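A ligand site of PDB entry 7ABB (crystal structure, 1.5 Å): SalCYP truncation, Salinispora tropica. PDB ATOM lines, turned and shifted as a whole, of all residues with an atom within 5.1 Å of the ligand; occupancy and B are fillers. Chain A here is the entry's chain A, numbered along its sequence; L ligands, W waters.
Phe 56 touches the ligand. Pro 80 touches the ligand. CA of Leu 81 touches O4 of the ligand (3.3 Å). CE1 of Phe 99 touches C26 of the ligand, 3.9 Å away. Leu 143 touches the ligand (CD1 to C26, 3.4 Å). Ala 235 touches the ligand. Gly 236 touches the ligand. Ser 239 touches the ligand (CB to C15, 3.6 Å). OG1 of Thr 240 touches C18 of the ligand (3.4 Å). His 243 touches the ligand (CD2 to C19, 3.2 Å). Leu 276 touches the ligand (CD2 to C19, 3.9 Å). Met 282 touches the ligand (SD to C2, 3.4 Å). CB of Pro 284 touches O1 of the ligand, 3.6 Å away. Leu 307 touches the ligand (CD1 to C9, 3.8 Å). Ala 334 touches the ligand. Phe 335 touches the ligand (CE1 to C15, 3.5 Å). Gly 336 touches the ligand. His 339 touches the ligand (O to O3, 3.9 Å). His 340 touches the ligand (CD2 to O4, 2.8 Å). Leu 343 touches the ligand (CB to C31, 3.8 Å). CA of Gly 344 touches C22 of the ligand, at 3.6 Å. Ala 348 touches the ligand. Hydrophobic or aromatic side chains that line the ligand: Phe 56, Pro 80, Leu 81, His 88, Phe 99, Leu 143, Ala 235, His 243, Leu 276, Met 282, Pro 284, Leu 307, Phe 335, His 340, Leu 343 and Ala 348. The nearest printed residue that does not touch the ligand is Leu 232 (4.03 Å).
Water W3 lies within hydrogen-bond range of O2 of the ligand (2.7 Å) and N of Gln 341 (3.4 Å). Water W4 bridges the backbone carbonyl oxygen (O) of Leu 81 and an oxygen (O1) of the ligand. Water W5 lies within hydrogen-bond range of O of Ala 334 and NE2 of His 243. Water W2 lies within hydrogen-bond range of the backbone carbonyl oxygen (O) of Ala 235, the side-chain hydroxyl (OG1) of Thr 240 and the backbone NH (N) of Ser 239.
ND1 of His 88 lies within hydrogen-bond range of O of Pro 80 (3.2 Å). The backbone carbonyl oxygen of Met 282 sits at hydrogen-bond distance from the backbone NH of Leu 307 (2.9 Å). The side-chain sulfur of Cys 342 lies close to the backbone NH of Gly 344 (3.2 Å). NE2 of His 340 sits at hydrogen-bond distance from O of Pro 80 (3.4 Å). The backbone carbonyl oxygen (O) of Phe 335 is in hydrogen-bond range of the backbone NH (N) of Cys 342. A ring nitrogen (NE2) of His 340 is in hydrogen-bond range of the backbone carbonyl oxygen (O) of Leu 81 (3.2 Å). ND1 of His 88 lies close to NE2 of His 340, at 3.4 Å. NE2 of His 88 sits at hydrogen-bond distance from O of His 339 (3.1 Å).
FE1 of the ligand is bound by SG of Cys 342 (2.3 Å). The guanidinium group (NH1) of Arg 92 lies within salt-bridge range of an oxygen (O3) of the ligand (2.6 Å). The guanidinium group (NH2) of Arg 286 is in salt-bridge range of an oxygen (O2) of the ligand (2.9 Å). NE2 of His 88 sits close to O3 of the ligand, 3.4 Å away.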
ATOM      1  N   PHE A  56       5.685 -28.846  30.079  1.00  0.00           N
ATOM      2  CA  PHE A  56       4.699 -28.631  29.023  1.00  0.00           C
ATOM      3  C   PHE A  56       5.092 -29.362  27.749  1.00  0.00           C
ATOM      4  O   PHE A  56       4.208 -29.769  26.977  1.00  0.00           O
ATOM      5  CB  PHE A  56       4.556 -27.141  28.703  1.00  0.00           C
ATOM      6  CG  PHE A  56       3.566 -26.385  29.571  1.00  0.00           C
ATOM      7  CD1 PHE A  56       2.214 -26.708  29.582  1.00  0.00           C
ATOM      8  CD2 PHE A  56       3.987 -25.320  30.354  1.00  0.00           C
ATOM      9  CE1 PHE A  56       1.306 -25.976  30.362  1.00  0.00           C
ATOM     10  CE2 PHE A  56       3.090 -24.602  31.120  1.00  0.00           C
ATOM     11  CZ  PHE A  56       1.759 -24.920  31.137  1.00  0.00           C
ATOM     12  N   PRO A  80     -10.112 -30.032  22.945  1.00  0.00           N
ATOM     13  CA  PRO A  80      -8.944 -30.915  22.848  1.00  0.00           C
ATOM     14  C   PRO A  80      -8.074 -30.947  24.100  1.00  0.00           C
ATOM     15  O   PRO A  80      -7.001 -31.520  24.078  1.00  0.00           O
ATOM     16  CB  PRO A  80      -8.158 -30.311  21.704  1.00  0.00           C
ATOM     17  CG  PRO A  80      -8.417 -28.828  21.835  1.00  0.00           C
ATOM     18  CD  PRO A  80      -9.806 -28.677  22.428  1.00  0.00           C
ATOM     19  N   LEU A  81      -8.550 -30.326  25.188  1.00  0.00           N
ATOM     20  CA  LEU A  81      -7.702 -30.033  26.343  1.00  0.00           C
ATOM     21  C   LEU A  81      -7.138 -31.298  27.003  1.00  0.00           C
ATOM     22  O   LEU A  81      -5.980 -31.311  27.442  1.00  0.00           O
ATOM     23  CB  LEU A  81      -8.529 -29.225  27.343  1.00  0.00           C
ATOM     24  CG  LEU A  81      -7.847 -28.524  28.518  1.00  0.00           C
ATOM     25  CD1 LEU A  81      -6.757 -27.548  28.071  1.00  0.00           C
ATOM     26  CD2 LEU A  81      -8.921 -27.800  29.314  1.00  0.00           C
ATOM     27  N   HIS A  88      -4.940 -35.901  19.414  1.00  0.00           N
ATOM     28  CA  HIS A  88      -4.897 -34.488  19.760  1.00  0.00           C
ATOM     29  C   HIS A  88      -4.283 -33.682  18.624  1.00  0.00           C
ATOM     30  O   HIS A  88      -4.777 -32.607  18.275  1.00  0.00           O
ATOM     31  CB  HIS A  88      -4.096 -34.262  21.036  1.00  0.00           C
ATOM     32  CG  HIS A  88      -3.784 -32.827  21.285  1.00  0.00           C
ATOM     33  ND1 HIS A  88      -4.645 -31.983  21.943  1.00  0.00           N
ATOM     34  CD2 HIS A  88      -2.709 -32.076  20.935  1.00  0.00           C
ATOM     35  CE1 HIS A  88      -4.109 -30.771  22.004  1.00  0.00           C
ATOM     36  NE2 HIS A  88      -2.944 -30.799  21.387  1.00  0.00           N
ATOM     37  N   ARG A  92      -6.027 -30.538  16.493  1.00  0.00           N
ATOM     38  CA  ARG A  92      -5.418 -29.226  16.333  1.00  0.00           C
ATOM     39  C   ARG A  92      -5.232 -28.896  14.847  1.00  0.00           C
ATOM     40  O   ARG A  92      -5.427 -27.742  14.446  1.00  0.00           O
ATOM     41  CB  ARG A  92      -4.088 -29.150  17.088  1.00  0.00           C
ATOM     42  CG  ARG A  92      -4.255 -29.117  18.617  1.00  0.00           C
ATOM     43  CD  ARG A  92      -4.992 -27.883  19.106  1.00  0.00           C
ATOM     44  NE  ARG A  92      -4.266 -26.646  18.815  1.00  0.00           N
ATOM     45  CZ  ARG A  92      -3.607 -25.924  19.729  1.00  0.00           C
ATOM     46  NH1 ARG A  92      -3.583 -26.315  20.997  1.00  0.00           N
ATOM     47  NH2 ARG A  92      -2.963 -24.820  19.379  1.00  0.00           N
ATOM     48  N   PHE A  99      -8.198 -20.258  13.778  1.00  0.00           N
ATOM     49  CA  PHE A  99      -7.482 -19.658  14.893  1.00  0.00           C
ATOM     50  C   PHE A  99      -6.075 -19.203  14.524  1.00  0.00           C
ATOM     51  O   PHE A  99      -5.237 -19.038  15.415  1.00  0.00           O
ATOM     52  CB  PHE A  99      -7.458 -20.639  16.059  1.00  0.00           C
ATOM     53  CG  PHE A  99      -8.815 -20.902  16.607  1.00  0.00           C
ATOM     54  CD1 PHE A  99      -9.433 -20.006  17.459  1.00  0.00           C
ATOM     55  CD2 PHE A  99      -9.519 -22.020  16.212  1.00  0.00           C
ATOM     56  CE1 PHE A  99     -10.725 -20.233  17.925  1.00  0.00           C
ATOM     57  CE2 PHE A  99     -10.826 -22.242  16.683  1.00  0.00           C
ATOM     58  CZ  PHE A  99     -11.405 -21.356  17.533  1.00  0.00           C
ATOM     59  N   LEU A 143     -15.778 -13.806  20.539  1.00  0.00           N
ATOM     60  CA  LEU A 143     -15.721 -15.276  20.550  1.00  0.00           C
ATOM     61  C   LEU A 143     -16.818 -15.858  19.675  1.00  0.00           C
ATOM     62  O   LEU A 143     -16.582 -16.751  18.855  1.00  0.00           O
ATOM     63  CB  LEU A 143     -15.873 -15.805  21.975  1.00  0.00           C
ATOM     64  CG  LEU A 143     -15.791 -17.325  22.146  1.00  0.00           C
ATOM     65  CD1 LEU A 143     -14.453 -17.859  21.726  1.00  0.00           C
ATOM     66  CD2 LEU A 143     -16.092 -17.725  23.584  1.00  0.00           C
ATOM     67  N   VAL A 231     -15.726 -26.464  25.354  1.00  0.00           N
ATOM     68  CA  VAL A 231     -14.385 -26.019  25.728  1.00  0.00           C
ATOM     69  C   VAL A 231     -14.101 -24.623  25.175  1.00  0.00           C
ATOM     70  O   VAL A 231     -13.544 -23.761  25.865  1.00  0.00           O
ATOM     71  CB  VAL A 231     -13.329 -27.034  25.240  1.00  0.00           C
ATOM     72  CG1 VAL A 231     -11.940 -26.446  25.313  1.00  0.00           C
ATOM     73  CG2 VAL A 231     -13.427 -28.303  26.043  1.00  0.00           C
ATOM     74  N   LEU A 232     -14.502 -24.377  23.929  1.00  0.00           N
ATOM     75  CA  LEU A 232     -14.284 -23.065  23.345  1.00  0.00           C
ATOM     76  C   LEU A 232     -14.995 -21.993  24.155  1.00  0.00           C
ATOM     77  O   LEU A 232     -14.431 -20.916  24.372  1.00  0.00           O
ATOM     78  CB  LEU A 232     -14.771 -23.045  21.901  1.00  0.00           C
ATOM     79  CG  LEU A 232     -13.877 -23.867  20.960  1.00  0.00           C
ATOM     80  CD1 LEU A 232     -14.484 -23.927  19.585  1.00  0.00           C
ATOM     81  CD2 LEU A 232     -12.493 -23.279  20.846  1.00  0.00           C
ATOM     82  N   ALA A 235     -13.066 -21.621  27.582  1.00  0.00           N
ATOM     83  CA  ALA A 235     -11.706 -21.105  27.435  1.00  0.00           C
ATOM     84  C   ALA A 235     -11.649 -19.694  26.878  1.00  0.00           C
ATOM     85  O   ALA A 235     -10.673 -18.973  27.119  1.00  0.00           O
ATOM     86  CB  ALA A 235     -10.909 -22.022  26.503  1.00  0.00           C
ATOM     87  N   GLY A 236     -12.668 -19.277  26.123  1.00  0.00           N
ATOM     88  CA  GLY A 236     -12.525 -18.119  25.263  1.00  0.00           C
ATOM     89  C   GLY A 236     -12.942 -16.758  25.801  1.00  0.00           C
ATOM     90  O   GLY A 236     -12.891 -15.819  25.023  1.00  0.00           O
ATOM     91  N   SER A 239     -10.142 -15.501  30.617  1.00  0.00           N
ATOM     92  CA  SER A 239      -8.728 -15.157  30.625  1.00  0.00           C
ATOM     93  C   SER A 239      -8.453 -13.884  29.824  1.00  0.00           C
ATOM     94  O   SER A 239      -7.616 -13.061  30.225  1.00  0.00           O
ATOM     95  CB  SER A 239      -7.876 -16.276  30.055  1.00  0.00           C
ATOM     96  OG  SER A 239      -7.712 -17.303  30.997  1.00  0.00           O
ATOM     97  N   THR A 240      -9.125 -13.726  28.678  1.00  0.00           N
ATOM     98  CA  THR A 240      -8.956 -12.522  27.866  1.00  0.00           C
ATOM     99  C   THR A 240      -9.479 -11.300  28.617  1.00  0.00           C
ATOM    100  O   THR A 240      -8.799 -10.276  28.671  1.00  0.00           O
ATOM    101  CB  THR A 240      -9.673 -12.677  26.516  1.00  0.00           C
ATOM    102  OG1 THR A 240      -9.233 -13.888  25.886  1.00  0.00           O
ATOM    103  CG2 THR A 240      -9.363 -11.525  25.590  1.00  0.00           C
ATOM    104  N   HIS A 243      -7.053 -10.406  31.520  1.00  0.00           N
ATOM    105  CA  HIS A 243      -5.845  -9.761  31.018  1.00  0.00           C
ATOM    106  C   HIS A 243      -6.123  -8.315  30.594  1.00  0.00           C
ATOM    107  O   HIS A 243      -5.327  -7.404  30.871  1.00  0.00           O
ATOM    108  CB  HIS A 243      -5.236 -10.567  29.874  1.00  0.00           C
ATOM    109  CG  HIS A 243      -4.230 -11.573  30.334  1.00  0.00           C
ATOM    110  ND1 HIS A 243      -3.010 -11.226  30.891  1.00  0.00           N
ATOM    111  CD2 HIS A 243      -4.266 -12.932  30.334  1.00  0.00           C
ATOM    112  CE1 HIS A 243      -2.330 -12.317  31.182  1.00  0.00           C
ATOM    113  NE2 HIS A 243      -3.072 -13.369  30.852  1.00  0.00           N
ATOM    114  N   LEU A 276       0.755  -9.607  29.301  1.00  0.00           N
ATOM    115  CA  LEU A 276       0.454 -11.039  29.328  1.00  0.00           C
ATOM    116  C   LEU A 276       1.393 -11.788  30.277  1.00  0.00           C
ATOM    117  O   LEU A 276       0.967 -12.658  31.062  1.00  0.00           O
ATOM    118  CB  LEU A 276       0.540 -11.617  27.911  1.00  0.00           C
ATOM    119  CG  LEU A 276      -0.616 -11.251  26.975  1.00  0.00           C
ATOM    120  CD1 LEU A 276      -0.257 -11.565  25.522  1.00  0.00           C
ATOM    121  CD2 LEU A 276      -1.858 -12.017  27.422  1.00  0.00           C
ATOM    122  N   MET A 282      -2.819 -18.688  35.338  1.00  0.00           N
ATOM    123  CA  MET A 282      -3.237 -20.080  35.225  1.00  0.00           C
ATOM    124  C   MET A 282      -2.193 -21.017  35.798  1.00  0.00           C
ATOM    125  O   MET A 282      -1.001 -20.710  35.860  1.00  0.00           O
ATOM    126  CB  MET A 282      -3.508 -20.461  33.777  1.00  0.00           C
ATOM    127  CG  MET A 282      -4.716 -19.764  33.230  1.00  0.00           C
ATOM    128  SD  MET A 282      -4.903 -19.933  31.438  1.00  0.00           S
ATOM    129  CE  MET A 282      -5.127 -21.685  31.286  1.00  0.00           C
ATOM    130  N   PRO A 284      -1.927 -24.818  34.880  1.00  0.00           N
ATOM    131  CA  PRO A 284      -2.265 -26.118  34.295  1.00  0.00           C
ATOM    132  C   PRO A 284      -1.634 -27.256  35.082  1.00  0.00           C
ATOM    133  O   PRO A 284      -0.504 -27.164  35.574  1.00  0.00           O
ATOM    134  CB  PRO A 284      -1.691 -26.025  32.883  1.00  0.00           C
ATOM    135  CG  PRO A 284      -1.702 -24.579  32.573  1.00  0.00           C
ATOM    136  CD  PRO A 284      -1.344 -23.905  33.880  1.00  0.00           C
ATOM    137  N   ARG A 286      -0.670 -31.510  35.387  1.00  0.00           N
ATOM    138  CA  ARG A 286      -0.273 -32.718  34.683  1.00  0.00           C
ATOM    139  C   ARG A 286      -0.114 -33.864  35.678  1.00  0.00           C
ATOM    140  O   ARG A 286       0.101 -33.650  36.872  1.00  0.00           O
ATOM    141  CB  ARG A 286       1.050 -32.513  33.934  1.00  0.00           C
ATOM    142  CG  ARG A 286       1.034 -31.386  32.888  1.00  0.00           C
ATOM    143  CD  ARG A 286       0.166 -31.727  31.759  1.00  0.00           C
ATOM    144  NE  ARG A 286       0.291 -30.877  30.581  1.00  0.00           N
ATOM    145  CZ  ARG A 286      -0.492 -29.832  30.307  1.00  0.00           C
ATOM    146  NH1 ARG A 286      -1.439 -29.467  31.165  1.00  0.00           N
ATOM    147  NH2 ARG A 286      -0.355 -29.192  29.143  1.00  0.00           N
ATOM    148  N   LEU A 307       1.904 -20.456  35.645  1.00  0.00           N
ATOM    149  CA  LEU A 307       2.487 -19.431  34.792  1.00  0.00           C
ATOM    150  C   LEU A 307       2.946 -18.214  35.609  1.00  0.00           C
ATOM    151  O   LEU A 307       3.846 -17.491  35.174  1.00  0.00           O
ATOM    152  CB  LEU A 307       1.470 -19.019  33.713  1.00  0.00           C
ATOM    153  CG  LEU A 307       0.920 -20.185  32.867  1.00  0.00           C
ATOM    154  CD1 LEU A 307       0.023 -19.607  31.783  1.00  0.00           C
ATOM    155  CD2 LEU A 307       2.060 -21.009  32.276  1.00  0.00           C
ATOM    156  N   ALA A 334       2.700 -17.059  28.597  1.00  0.00           N
ATOM    157  CA  ALA A 334       1.349 -16.748  29.046  1.00  0.00           C
ATOM    158  C   ALA A 334       0.323 -17.657  28.432  1.00  0.00           C
ATOM    159  O   ALA A 334      -0.776 -17.810  28.995  1.00  0.00           O
ATOM    160  CB  ALA A 334       1.011 -15.302  28.699  1.00  0.00           C
ATOM    161  N   PHE A 335       0.622 -18.221  27.263  1.00  0.00           N
ATOM    162  CA  PHE A 335      -0.302 -19.099  26.552  1.00  0.00           C
ATOM    163  C   PHE A 335       0.126 -20.555  26.627  1.00  0.00           C
ATOM    164  O   PHE A 335      -0.331 -21.383  25.827  1.00  0.00           O
ATOM    165  CB  PHE A 335      -0.402 -18.670  25.090  1.00  0.00           C
ATOM    166  CG  PHE A 335      -1.083 -17.331  24.900  1.00  0.00           C
ATOM    167  CD1 PHE A 335      -2.429 -17.177  25.149  1.00  0.00           C
ATOM    168  CD2 PHE A 335      -0.341 -16.250  24.474  1.00  0.00           C
ATOM    169  CE1 PHE A 335      -3.047 -15.952  24.957  1.00  0.00           C
ATOM    170  CE2 PHE A 335      -0.947 -15.016  24.268  1.00  0.00           C
ATOM    171  CZ  PHE A 335      -2.299 -14.866  24.525  1.00  0.00           C
ATOM    172  N   GLY A 336       1.004 -20.909  27.559  1.00  0.00           N
ATOM    173  CA  GLY A 336       1.551 -22.226  27.614  1.00  0.00           C
ATOM    174  C   GLY A 336       2.594 -22.465  26.539  1.00  0.00           C
ATOM    175  O   GLY A 336       3.050 -21.553  25.844  1.00  0.00           O
ATOM    176  N   HIS A 339       2.360 -29.015  23.072  1.00  0.00           N
ATOM    177  CA  HIS A 339       1.298 -29.364  22.122  1.00  0.00           C
ATOM    178  C   HIS A 339      -0.027 -28.738  22.478  1.00  0.00           C
ATOM    179  O   HIS A 339      -0.872 -28.536  21.598  1.00  0.00           O
ATOM    180  CB  HIS A 339       1.134 -30.873  22.073  1.00  0.00           C
ATOM    181  CG  HIS A 339       2.254 -31.560  21.363  1.00  0.00           C
ATOM    182  ND1 HIS A 339       2.777 -31.102  20.178  1.00  0.00           N
ATOM    183  CD2 HIS A 339       2.962 -32.664  21.683  1.00  0.00           C
ATOM    184  CE1 HIS A 339       3.748 -31.911  19.784  1.00  0.00           C
ATOM    185  NE2 HIS A 339       3.889 -32.866  20.691  1.00  0.00           N
ATOM    186  N   HIS A 340      -0.258 -28.423  23.753  1.00  0.00           N
ATOM    187  CA  HIS A 340      -1.518 -27.851  24.187  1.00  0.00           C
ATOM    188  C   HIS A 340      -1.514 -26.323  24.245  1.00  0.00           C
ATOM    189  O   HIS A 340      -2.485 -25.713  24.735  1.00  0.00           O
ATOM    190  CB  HIS A 340      -1.917 -28.465  25.536  1.00  0.00           C
ATOM    191  CG  HIS A 340      -2.476 -29.835  25.407  1.00  0.00           C
ATOM    192  ND1 HIS A 340      -1.697 -30.982  25.380  1.00  0.00           N
ATOM    193  CD2 HIS A 340      -3.748 -30.263  25.253  1.00  0.00           C
ATOM    194  CE1 HIS A 340      -2.479 -32.033  25.229  1.00  0.00           C
ATOM    195  NE2 HIS A 340      -3.731 -31.627  25.153  1.00  0.00           N
ATOM    196  N   GLN A 341      -0.468 -25.683  23.723  1.00  0.00           N
ATOM    197  CA  GLN A 341      -0.357 -24.227  23.726  1.00  0.00           C
ATOM    198  C   GLN A 341      -1.647 -23.600  23.185  1.00  0.00           C
ATOM    199  O   GLN A 341      -2.217 -24.089  22.209  1.00  0.00           O
ATOM    200  CB  GLN A 341       0.837 -23.816  22.853  1.00  0.00           C
ATOM    201  CG  GLN A 341       1.237 -22.337  22.862  1.00  0.00           C
ATOM    202  CD  GLN A 341       2.345 -22.093  21.838  1.00  0.00           C
ATOM    203  OE1 GLN A 341       2.099 -22.083  20.637  1.00  0.00           O
ATOM    204  NE2 GLN A 341       3.567 -21.963  22.327  1.00  0.00           N
ATOM    205  N   CYS A 342      -2.102 -22.536  23.816  1.00  0.00           N
ATOM    206  CA  CYS A 342      -3.429 -21.962  23.580  1.00  0.00           C
ATOM    207  C   CYS A 342      -3.794 -21.839  22.095  1.00  0.00           C
ATOM    208  O   CYS A 342      -3.091 -21.174  21.328  1.00  0.00           O
ATOM    209  CB  CYS A 342      -3.495 -20.586  24.223  1.00  0.00           C
ATOM    210  SG  CYS A 342      -5.092 -19.776  24.007  1.00  0.00           S
ATOM    211  N   LEU A 343      -4.942 -22.433  21.734  1.00  0.00           N
ATOM    212  CA  LEU A 343      -5.472 -22.303  20.376  1.00  0.00           C
ATOM    213  C   LEU A 343      -5.857 -20.868  20.055  1.00  0.00           C
ATOM    214  O   LEU A 343      -5.756 -20.428  18.902  1.00  0.00           O
ATOM    215  CB  LEU A 343      -6.693 -23.214  20.264  1.00  0.00           C
ATOM    216  CG  LEU A 343      -7.426 -23.288  18.920  1.00  0.00           C
ATOM    217  CD1 LEU A 343      -6.545 -23.924  17.852  1.00  0.00           C
ATOM    218  CD2 LEU A 343      -8.689 -24.113  19.119  1.00  0.00           C
ATOM    219  N   GLY A 344      -6.306 -20.139  21.045  1.00  0.00           N
ATOM    220  CA  GLY A 344      -6.832 -18.794  20.868  1.00  0.00           C
ATOM    221  C   GLY A 344      -5.824 -17.678  21.041  1.00  0.00           C
ATOM    222  O   GLY A 344      -6.240 -16.517  21.126  1.00  0.00           O
ATOM    223  N   TYR A 347      -5.971 -14.740  18.633  1.00  0.00           N
ATOM    224  CA  TYR A 347      -7.249 -14.033  18.737  1.00  0.00           C
ATOM    225  C   TYR A 347      -7.289 -13.218  20.018  1.00  0.00           C
ATOM    226  O   TYR A 347      -7.803 -12.098  20.017  1.00  0.00           O
ATOM    227  CB  TYR A 347      -8.420 -15.025  18.675  1.00  0.00           C
ATOM    228  CG  TYR A 347      -9.737 -14.403  18.250  1.00  0.00           C
ATOM    229  CD1 TYR A 347      -9.820 -13.699  17.074  1.00  0.00           C
ATOM    230  CD2 TYR A 347     -10.883 -14.560  18.999  1.00  0.00           C
ATOM    231  CE1 TYR A 347     -11.003 -13.129  16.655  1.00  0.00           C
ATOM    232  CE2 TYR A 347     -12.091 -14.003  18.596  1.00  0.00           C
ATOM    233  CZ  TYR A 347     -12.133 -13.286  17.418  1.00  0.00           C
ATOM    234  OH  TYR A 347     -13.317 -12.718  16.969  1.00  0.00           O
ATOM    235  N   ALA A 348      -6.807 -13.793  21.110  1.00  0.00           N
ATOM    236  CA  ALA A 348      -6.723 -13.050  22.379  1.00  0.00           C
ATOM    237  C   ALA A 348      -5.852 -11.822  22.226  1.00  0.00           C
ATOM    238  O   ALA A 348      -6.235 -10.720  22.655  1.00  0.00           O
ATOM    239  CB  ALA A 348      -6.190 -13.966  23.483  1.00  0.00           C
ATOM    240  N   GLN A 351      -7.689  -9.152  20.336  1.00  0.00           N
ATOM    241  CA  GLN A 351      -8.738  -8.514  21.117  1.00  0.00           C
ATOM    242  C   GLN A 351      -8.175  -7.527  22.137  1.00  0.00           C
ATOM    243  O   GLN A 351      -8.758  -6.448  22.352  1.00  0.00           O
ATOM    244  CB  GLN A 351      -9.566  -9.562  21.844  1.00  0.00           C
ATOM    245  CG  GLN A 351     -10.424 -10.407  20.938  1.00  0.00           C
ATOM    246  CD  GLN A 351     -11.195 -11.411  21.707  1.00  0.00           C
ATOM    247  OE1 GLN A 351     -12.179 -11.074  22.338  1.00  0.00           O
ATOM    248  NE2 GLN A 351     -10.738 -12.669  21.682  1.00  0.00           N
ATOM    249  N   ILE A 352      -7.085  -7.898  22.820  1.00  0.00           N
ATOM    250  CA  ILE A 352      -6.504  -7.041  23.850  1.00  0.00           C
ATOM    251  C   ILE A 352      -5.941  -5.781  23.217  1.00  0.00           C
ATOM    252  O   ILE A 352      -6.251  -4.655  23.634  1.00  0.00           O
ATOM    253  CB  ILE A 352      -5.429  -7.812  24.628  1.00  0.00           C
ATOM    254  CG1 ILE A 352      -6.071  -8.922  25.425  1.00  0.00           C
ATOM    255  CG2 ILE A 352      -4.681  -6.886  25.592  1.00  0.00           C
ATOM    256  CD1 ILE A 352      -5.049  -9.977  25.913  1.00  0.00           C
HETATM  257 FE1  LIG L   1      -6.410 -20.420  25.741  1.00  0.00          FE
HETATM  258  C1  LIG L   1      -5.311 -23.665  26.063  1.00  0.00           C
HETATM  259  C2  LIG L   1      -4.141 -19.485  28.135  1.00  0.00           C
HETATM  260  C3  LIG L   1      -7.472 -17.175  25.421  1.00  0.00           C
HETATM  261  C4  LIG L   1      -8.907 -21.415  23.650  1.00  0.00           C
HETATM  262  N1  LIG L   1      -5.041 -21.378  26.870  1.00  0.00           N
HETATM  263  C5  LIG L   1      -4.685 -22.723  26.827  1.00  0.00           C
HETATM  264  C6  LIG L   1      -3.576 -23.013  27.727  1.00  0.00           C
HETATM  265  C7  LIG L   1      -3.265 -21.830  28.280  1.00  0.00           C
HETATM  266  C8  LIG L   1      -4.151 -20.816  27.765  1.00  0.00           C
HETATM  267  C9  LIG L   1      -2.179 -21.542  29.327  1.00  0.00           C
HETATM  268  C10 LIG L   1      -2.879 -24.402  27.945  1.00  0.00           C
HETATM  269  C11 LIG L   1      -3.519 -25.253  29.033  1.00  0.00           C
HETATM  270  C12 LIG L   1      -2.729 -26.543  29.200  1.00  0.00           C
HETATM  271  O1  LIG L   1      -3.242 -27.370  29.983  1.00  0.00           O
HETATM  272  O2  LIG L   1      -1.652 -26.676  28.565  1.00  0.00           O
HETATM  273  N2  LIG L   1      -5.953 -18.685  26.645  1.00  0.00           N
HETATM  274  C13 LIG L   1      -4.944 -18.488  27.579  1.00  0.00           C
HETATM  275  C14 LIG L   1      -4.880 -17.086  27.850  1.00  0.00           C
HETATM  276  C15 LIG L   1      -5.780 -16.454  27.076  1.00  0.00           C
HETATM  277  C16 LIG L   1      -6.483 -17.434  26.328  1.00  0.00           C
HETATM  278  C17 LIG L   1      -3.844 -16.521  28.850  1.00  0.00           C
HETATM  279  C18 LIG L   1      -6.178 -15.010  26.933  1.00  0.00           C
HETATM  280  C19 LIG L   1      -5.239 -13.997  27.496  1.00  0.00           C
HETATM  281  N3  LIG L   1      -7.924 -19.494  24.745  1.00  0.00           N
HETATM  282  C20 LIG L   1      -8.121 -18.134  24.685  1.00  0.00           C
HETATM  283  C21 LIG L   1      -9.156 -17.856  23.724  1.00  0.00           C
HETATM  284  C22 LIG L   1      -9.577 -19.035  23.198  1.00  0.00           C
HETATM  285  C23 LIG L   1      -8.811 -20.060  23.863  1.00  0.00           C
HETATM  286  C24 LIG L   1      -9.632 -16.447  23.373  1.00  0.00           C
HETATM  287  C25 LIG L   1     -10.668 -19.354  22.172  1.00  0.00           C
HETATM  288  C26 LIG L   1     -11.156 -18.260  21.221  1.00  0.00           C
HETATM  289  N4  LIG L   1      -6.998 -22.194  25.033  1.00  0.00           N
HETATM  290  C27 LIG L   1      -8.067 -22.352  24.158  1.00  0.00           C
HETATM  291  C28 LIG L   1      -8.166 -23.745  23.835  1.00  0.00           C
HETATM  292  C29 LIG L   1      -7.080 -24.465  24.568  1.00  0.00           C
HETATM  293  C30 LIG L   1      -6.379 -23.414  25.271  1.00  0.00           C
HETATM  294  C31 LIG L   1      -9.217 -24.366  22.918  1.00  0.00           C
HETATM  295  C32 LIG L   1      -6.764 -25.964  24.557  1.00  0.00           C
HETATM  296  C33 LIG L   1      -5.740 -26.216  23.474  1.00  0.00           C
HETATM  297  C34 LIG L   1      -5.311 -27.670  23.482  1.00  0.00           C
HETATM  298  O3  LIG L   1      -4.694 -28.122  22.492  1.00  0.00           O
HETATM  299  O4  LIG L   1      -5.589 -28.341  24.501  1.00  0.00           O
HETATM  300  O   HOH W   1      -5.118 -26.623  31.725  1.00  0.00           O
HETATM  301  O   HOH W   2     -10.104 -16.234  27.233  1.00  0.00           O
HETATM  302  O   HOH W   3       0.243 -25.466  27.042  1.00  0.00           O
HETATM  303  O   HOH W   4      -4.464 -29.885  29.197  1.00  0.00           O
HETATM  304  O   HOH W   5      -1.411 -15.975  30.954  1.00  0.00           O
